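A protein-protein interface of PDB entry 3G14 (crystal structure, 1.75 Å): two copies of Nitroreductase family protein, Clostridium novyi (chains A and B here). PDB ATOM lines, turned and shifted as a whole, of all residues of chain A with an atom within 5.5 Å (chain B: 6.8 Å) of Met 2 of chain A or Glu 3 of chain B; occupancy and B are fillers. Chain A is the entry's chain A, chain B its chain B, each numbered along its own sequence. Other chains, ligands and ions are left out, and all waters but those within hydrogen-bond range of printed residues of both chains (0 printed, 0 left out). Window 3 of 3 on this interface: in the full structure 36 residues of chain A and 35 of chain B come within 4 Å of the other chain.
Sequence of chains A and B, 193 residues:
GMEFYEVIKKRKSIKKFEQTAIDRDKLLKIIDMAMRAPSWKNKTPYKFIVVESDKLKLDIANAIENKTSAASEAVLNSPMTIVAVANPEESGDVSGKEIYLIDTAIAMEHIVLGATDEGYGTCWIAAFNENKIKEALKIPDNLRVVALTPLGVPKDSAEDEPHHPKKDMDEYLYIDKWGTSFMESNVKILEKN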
ATOM      1  N   MET A   2      14.049   8.595 -18.611  1.00  0.00           N
ATOM      2  CA  MET A   2      14.617   7.431 -19.351  1.00  0.00           C
ATOM      3  C   MET A   2      15.754   7.872 -20.265  1.00  0.00           C
ATOM      4  O   MET A   2      15.706   8.970 -20.857  1.00  0.00           O
ATOM      5  CB  MET A   2      13.549   6.765 -20.217  1.00  0.00           C
ATOM      6  CG  MET A   2      12.349   6.241 -19.458  1.00  0.00           C
ATOM      7  SD  MET A   2      11.213   5.216 -20.617  1.00  0.00           S
ATOM      8  CE  MET A   2      12.443   3.882 -21.190  1.00  0.00           C
ATOM      9  N   GLU A   3      16.739   6.996 -20.418  1.00  0.00           N
ATOM     10  CA  GLU A   3      17.843   7.215 -21.358  1.00  0.00           C
ATOM     11  C   GLU A   3      17.314   7.110 -22.774  1.00  0.00           C
ATOM     12  O   GLU A   3      16.364   6.365 -23.033  1.00  0.00           O
ATOM     13  CB  GLU A   3      18.951   6.177 -21.171  1.00  0.00           C
ATOM     14  CG  GLU A   3      20.333   6.560 -21.768  1.00  0.00           C
ATOM     15  CD  GLU A   3      20.598   5.950 -23.163  1.00  0.00           C
ATOM     16  OE1 GLU A   3      20.609   4.694 -23.227  1.00  0.00           O
ATOM     17  OE2 GLU A   3      20.809   6.709 -24.171  1.00  0.00           O
ATOM     18  N   PHE A   4      17.945   7.851 -23.682  1.00  0.00           N
ATOM     19  CA  PHE A   4      17.469   7.887 -25.051  1.00  0.00           C
ATOM     20  C   PHE A   4      17.381   6.512 -25.706  1.00  0.00           C
ATOM     21  O   PHE A   4      16.348   6.138 -26.266  1.00  0.00           O
ATOM     22  CB  PHE A   4      18.319   8.822 -25.928  1.00  0.00           C
ATOM     23  CG  PHE A   4      17.749   8.995 -27.311  1.00  0.00           C
ATOM     24  CD1 PHE A   4      16.707   9.906 -27.555  1.00  0.00           C
ATOM     25  CD2 PHE A   4      18.199   8.209 -28.363  1.00  0.00           C
ATOM     26  CE1 PHE A   4      16.152  10.022 -28.845  1.00  0.00           C
ATOM     27  CE2 PHE A   4      17.642   8.340 -29.627  1.00  0.00           C
ATOM     28  CZ  PHE A   4      16.632   9.231 -29.854  1.00  0.00           C
ATOM     29  N   GLU A   6      17.168   3.677 -24.390  1.00  0.00           N
ATOM     30  CA  GLU A   6      16.183   2.839 -23.710  1.00  0.00           C
ATOM     31  C   GLU A   6      14.772   3.102 -24.230  1.00  0.00           C
ATOM     32  O   GLU A   6      13.991   2.170 -24.375  1.00  0.00           O
ATOM     33  CB  GLU A   6      16.254   3.029 -22.194  1.00  0.00           C
ATOM     34  CG  GLU A   6      15.370   2.076 -21.428  1.00  0.00           C
ATOM     35  CD  GLU A   6      15.844   0.620 -21.476  1.00  0.00           C
ATOM     36  OE1 GLU A   6      16.976   0.334 -21.966  1.00  0.00           O
ATOM     37  OE2 GLU A   6      15.073  -0.238 -20.986  1.00  0.00           O
ATOM     38  N   VAL A   7      14.437   4.368 -24.489  1.00  0.00           N
ATOM     39  CA  VAL A   7      13.150   4.737 -25.123  1.00  0.00           C
ATOM     40  C   VAL A   7      13.008   4.097 -26.514  1.00  0.00           C
ATOM     41  O   VAL A   7      12.014   3.474 -26.839  1.00  0.00           O
ATOM     42  CB  VAL A   7      13.004   6.269 -25.203  1.00  0.00           C
ATOM     43  CG1 VAL A   7      11.702   6.688 -25.951  1.00  0.00           C
ATOM     44  CG2 VAL A   7      13.112   6.910 -23.782  1.00  0.00           C
ATOM     45  N   LYS A  10      12.327   0.447 -25.932  1.00  0.00           N
ATOM     46  CA  LYS A  10      11.066   0.194 -25.233  1.00  0.00           C
ATOM     47  C   LYS A  10       9.849   0.459 -26.109  1.00  0.00           C
ATOM     48  O   LYS A  10       8.799  -0.119 -25.883  1.00  0.00           O
ATOM     49  CB  LYS A  10      10.993   1.052 -23.964  1.00  0.00           C
ATOM     50  CG  LYS A  10       9.683   0.945 -23.181  1.00  0.00           C
ATOM     51  CD  LYS A  10       9.866   1.380 -21.726  1.00  0.00           C
ATOM     52  CE  LYS A  10       8.657   1.069 -20.832  1.00  0.00           C
ATOM     53  NZ  LYS A  10       8.363  -0.383 -20.684  1.00  0.00           N
ATOM     54  N   THR A 116       6.395   7.234 -25.229  1.00  0.00           N
ATOM     55  CA  THR A 116       7.100   6.117 -24.600  1.00  0.00           C
ATOM     56  C   THR A 116       7.938   6.593 -23.406  1.00  0.00           C
ATOM     57  O   THR A 116       7.925   5.951 -22.340  1.00  0.00           O
ATOM     58  CB  THR A 116       8.021   5.386 -25.643  1.00  0.00           C
ATOM     59  OG1 THR A 116       7.246   4.989 -26.804  1.00  0.00           O
ATOM     60  CG2 THR A 116       8.747   4.223 -25.013  1.00  0.00           C
ATOM     61  N   ASP A 117       8.676   7.698 -23.604  1.00  0.00           N
ATOM     62  CA  ASP A 117       9.441   8.375 -22.554  1.00  0.00           C
ATOM     63  C   ASP A 117       8.570   8.701 -21.342  1.00  0.00           C
ATOM     64  O   ASP A 117       9.004   8.530 -20.191  1.00  0.00           O
ATOM     65  CB  ASP A 117      10.029   9.672 -23.106  1.00  0.00           C
ATOM     66  CG  ASP A 117      10.865  10.422 -22.096  1.00  0.00           C
ATOM     67  OD1 ASP A 117      11.880   9.870 -21.618  1.00  0.00           O
ATOM     68  OD2 ASP A 117      10.488  11.560 -21.778  1.00  0.00           O
ATOM     69  N   MET B   2      22.785   9.785 -23.141  1.00  0.00           N
ATOM     70  CA  MET B   2      21.963  10.969 -22.735  1.00  0.00           C
ATOM     71  C   MET B   2      20.516  10.643 -22.409  1.00  0.00           C
ATOM     72  O   MET B   2      19.948   9.649 -22.882  1.00  0.00           O
ATOM     73  CB  MET B   2      21.948  12.013 -23.847  1.00  0.00           C
ATOM     74  CG  MET B   2      23.279  12.568 -24.197  1.00  0.00           C
ATOM     75  SD  MET B   2      23.088  13.821 -25.631  1.00  0.00           S
ATOM     76  CE  MET B   2      21.933  15.113 -24.845  1.00  0.00           C
ATOM     77  N   GLU B   3      19.923  11.507 -21.590  1.00  0.00           N
ATOM     78  CA  GLU B   3      18.507  11.436 -21.282  1.00  0.00           C
ATOM     79  C   GLU B   3      17.617  11.805 -22.502  1.00  0.00           C
ATOM     80  O   GLU B   3      17.996  12.623 -23.327  1.00  0.00           O
ATOM     81  CB  GLU B   3      18.233  12.330 -20.089  1.00  0.00           C
ATOM     82  CG  GLU B   3      16.831  12.220 -19.542  1.00  0.00           C
ATOM     83  CD  GLU B   3      15.873  13.159 -20.245  1.00  0.00           C
ATOM     84  OE1 GLU B   3      16.323  14.303 -20.551  1.00  0.00           O
ATOM     85  OE2 GLU B   3      14.702  12.746 -20.493  1.00  0.00           O
ATOM     86  N   PHE B   4      16.437  11.190 -22.608  1.00  0.00           N
ATOM     87  CA  PHE B   4      15.662  11.265 -23.832  1.00  0.00           C
ATOM     88  C   PHE B   4      15.296  12.702 -24.228  1.00  0.00           C
ATOM     89  O   PHE B   4      15.576  13.132 -25.334  1.00  0.00           O
ATOM     90  CB  PHE B   4      14.372  10.408 -23.746  1.00  0.00           C
ATOM     91  CG  PHE B   4      13.527  10.537 -24.963  1.00  0.00           C
ATOM     92  CD1 PHE B   4      13.798   9.789 -26.088  1.00  0.00           C
ATOM     93  CD2 PHE B   4      12.489  11.469 -25.013  1.00  0.00           C
ATOM     94  CE1 PHE B   4      13.054   9.964 -27.235  1.00  0.00           C
ATOM     95  CE2 PHE B   4      11.746  11.612 -26.163  1.00  0.00           C
ATOM     96  CZ  PHE B   4      12.030  10.866 -27.248  1.00  0.00           C
ATOM     97  N   TYR B   5      14.670  13.454 -23.319  1.00  0.00           N
ATOM     98  CA  TYR B   5      14.244  14.816 -23.632  1.00  0.00           C
ATOM     99  C   TYR B   5      15.452  15.724 -23.954  1.00  0.00           C
ATOM    100  O   TYR B   5      15.391  16.564 -24.868  1.00  0.00           O
ATOM    101  CB  TYR B   5      13.397  15.365 -22.477  1.00  0.00           C
ATOM    102  CG  TYR B   5      12.528  16.578 -22.774  1.00  0.00           C
ATOM    103  CD1 TYR B   5      12.145  16.935 -24.079  1.00  0.00           C
ATOM    104  CD2 TYR B   5      12.030  17.341 -21.725  1.00  0.00           C
ATOM    105  CE1 TYR B   5      11.306  18.045 -24.320  1.00  0.00           C
ATOM    106  CE2 TYR B   5      11.204  18.437 -21.949  1.00  0.00           C
ATOM    107  CZ  TYR B   5      10.845  18.787 -23.242  1.00  0.00           C
ATOM    108  OH  TYR B   5      10.036  19.892 -23.395  1.00  0.00           O
ATOM    109  N   GLU B   6      16.569  15.506 -23.256  1.00  0.00           N
ATOM    110  CA  GLU B   6      17.823  16.218 -23.558  1.00  0.00           C
ATOM    111  C   GLU B   6      18.288  15.958 -24.979  1.00  0.00           C
ATOM    112  O   GLU B   6      18.842  16.841 -25.619  1.00  0.00           O
ATOM    113  CB  GLU B   6      18.945  15.835 -22.584  1.00  0.00           C
ATOM    114  CG  GLU B   6      18.809  16.452 -21.215  1.00  0.00           C
ATOM    115  CD  GLU B   6      18.592  17.960 -21.282  1.00  0.00           C
ATOM    116  OE1 GLU B   6      19.382  18.631 -21.985  1.00  0.00           O
ATOM    117  OE2 GLU B   6      17.631  18.465 -20.647  1.00  0.00           O
ATOM    118  N   VAL B   7      18.081  14.744 -25.484  1.00  0.00           N
ATOM    119  CA  VAL B   7      18.461  14.464 -26.881  1.00  0.00           C
ATOM    120  C   VAL B   7      17.585  15.292 -27.833  1.00  0.00           C
ATOM    121  O   VAL B   7      18.052  15.923 -28.797  1.00  0.00           O
ATOM    122  CB  VAL B   7      18.430  12.952 -27.221  1.00  0.00           C
ATOM    123  CG1 VAL B   7      18.673  12.720 -28.715  1.00  0.00           C
ATOM    124  CG2 VAL B   7      19.451  12.177 -26.385  1.00  0.00           C
ATOM    125  N   ILE B   8      16.295  15.342 -27.544  1.00  0.00           N
ATOM    126  CA  ILE B   8      15.378  16.081 -28.414  1.00  0.00           C
ATOM    127  C   ILE B   8      15.760  17.567 -28.440  1.00  0.00           C
ATOM    128  O   ILE B   8      15.722  18.189 -29.492  1.00  0.00           O
ATOM    129  CB  ILE B   8      13.898  15.929 -27.921  1.00  0.00           C
ATOM    130  CG1 ILE B   8      13.532  14.437 -27.903  1.00  0.00           C
ATOM    131  CG2 ILE B   8      12.923  16.821 -28.769  1.00  0.00           C
ATOM    132  CD1 ILE B   8      13.506  13.720 -29.286  1.00  0.00           C
ATOM    133  N   ASP B 117      22.425  11.715 -29.650  1.00  0.00           N
ATOM    134  CA  ASP B 117      22.701  10.891 -28.457  1.00  0.00           C
ATOM    135  C   ASP B 117      24.154  10.425 -28.343  1.00  0.00           C
ATOM    136  O   ASP B 117      24.674  10.325 -27.226  1.00  0.00           O
ATOM    137  CB  ASP B 117      21.722   9.690 -28.467  1.00  0.00           C
ATOM    138  CG  ASP B 117      21.917   8.744 -27.321  1.00  0.00           C
ATOM    139  OD1 ASP B 117      21.722   9.155 -26.173  1.00  0.00           O
ATOM    140  OD2 ASP B 117      22.271   7.578 -27.580  1.00  0.00           O
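The side-chain carboxylate (OE2) of Glu 3 of chain A sits close to the side-chain carboxylate (OD1) of Asp 117 of chain B, at 3.3 Å. The side-chain carboxylate of Glu 3 of chain A lies close to the backbone carbonyl oxygen of Met 2 of chain B. The backbone carbonyl oxygen (O) of Met 2 of chain B lies within hydrogen-bond range of the backbone NH (N) of Phe 4 of chain A (2.8 Å). The backbone NH of Phe 4 of chain B sits at hydrogen-bond distance from the backbone carbonyl oxygen of Met 2 of chain A.
The backbone NH (N) of Glu 6 of chain B sits at hydrogen-bond distance from the side-chain carboxylate (OE1) of Glu 3 of chain B. OE2 of Glu 3 of chain B is in hydrogen-bond range of N of Tyr 5 of chain B (2.9 Å). N of Met 2 of chain B lies within hydrogen-bond range of OD1 of Asp 117 of chain B.
Met 2 of chain A touches Glu 3 of chain B (O to CG, 3.7 Å). CD1 of Phe 4 of chain B touches CD1 of Phe 4 of chain A, at 3.3 Å. Val 7 of chain B touches Phe 4 of chain A (CB to CD1, 3.5 Å). CB of Phe 4 of chain A touches OD1 of Asp 117 of chain B, at 3.4 Å. Val 7 of chain A touches Phe 4 of chain B (CB to CD1, 3.7 Å). OD1 of Asp 117 of chain A touches CB of Phe 4 of chain B, 3.3 Å away.
Met 2 of chain A touches just these residues of chain B: Glu 3 and Phe 4. Glu 3 of chain B touches one residue of chain A. Of the printed residues of chain B, Glu 3 of chain A touches Met 2 and Asp 117. Printed residues of chain B within 4 Å of Asp 117 of chain A: Phe 4. Printed residues of chain A within 4 Å of Phe 4 of chain B: Met 2, Phe 4, Val 7 and Asp 117. Printed residues of chain A within 4 Å of Met 2 of chain B: Glu 3 (3.3 Å) and Phe 4 (2.8 Å). Glu 6 of chain B touches none of the printed residues of chain A.
Printed residues of chain A that touch a printed residue of chain B: Met 2, Glu 3, Phe 4, Val 7 and Asp 117. Along chain A the printed residues that touch a printed residue of chain B span positions 2 to 117. Among the printed residues, no Asp or Glu carboxylate lies within 4 Å of a Lys or Arg side-chain nitrogen of the other chain.
Met 2 of chain A touches Glu 3 of chain B, and with the chains exchanged Glu 3 of chain A touches Met 2 of chain B. Met 2 of chain A touches Phe 4 of chain B, and with the chains exchanged Phe 4 of chain A touches Met 2 of chain B. Phe 4 of chain B touches its own counterpart, Phe 4 of chain A. Phe 4 of chain A touches Asp 117 of chain B, and with the chains exchanged Asp 117 of chain A touches Phe 4 of chain B. 6 positions are printed for both chains.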
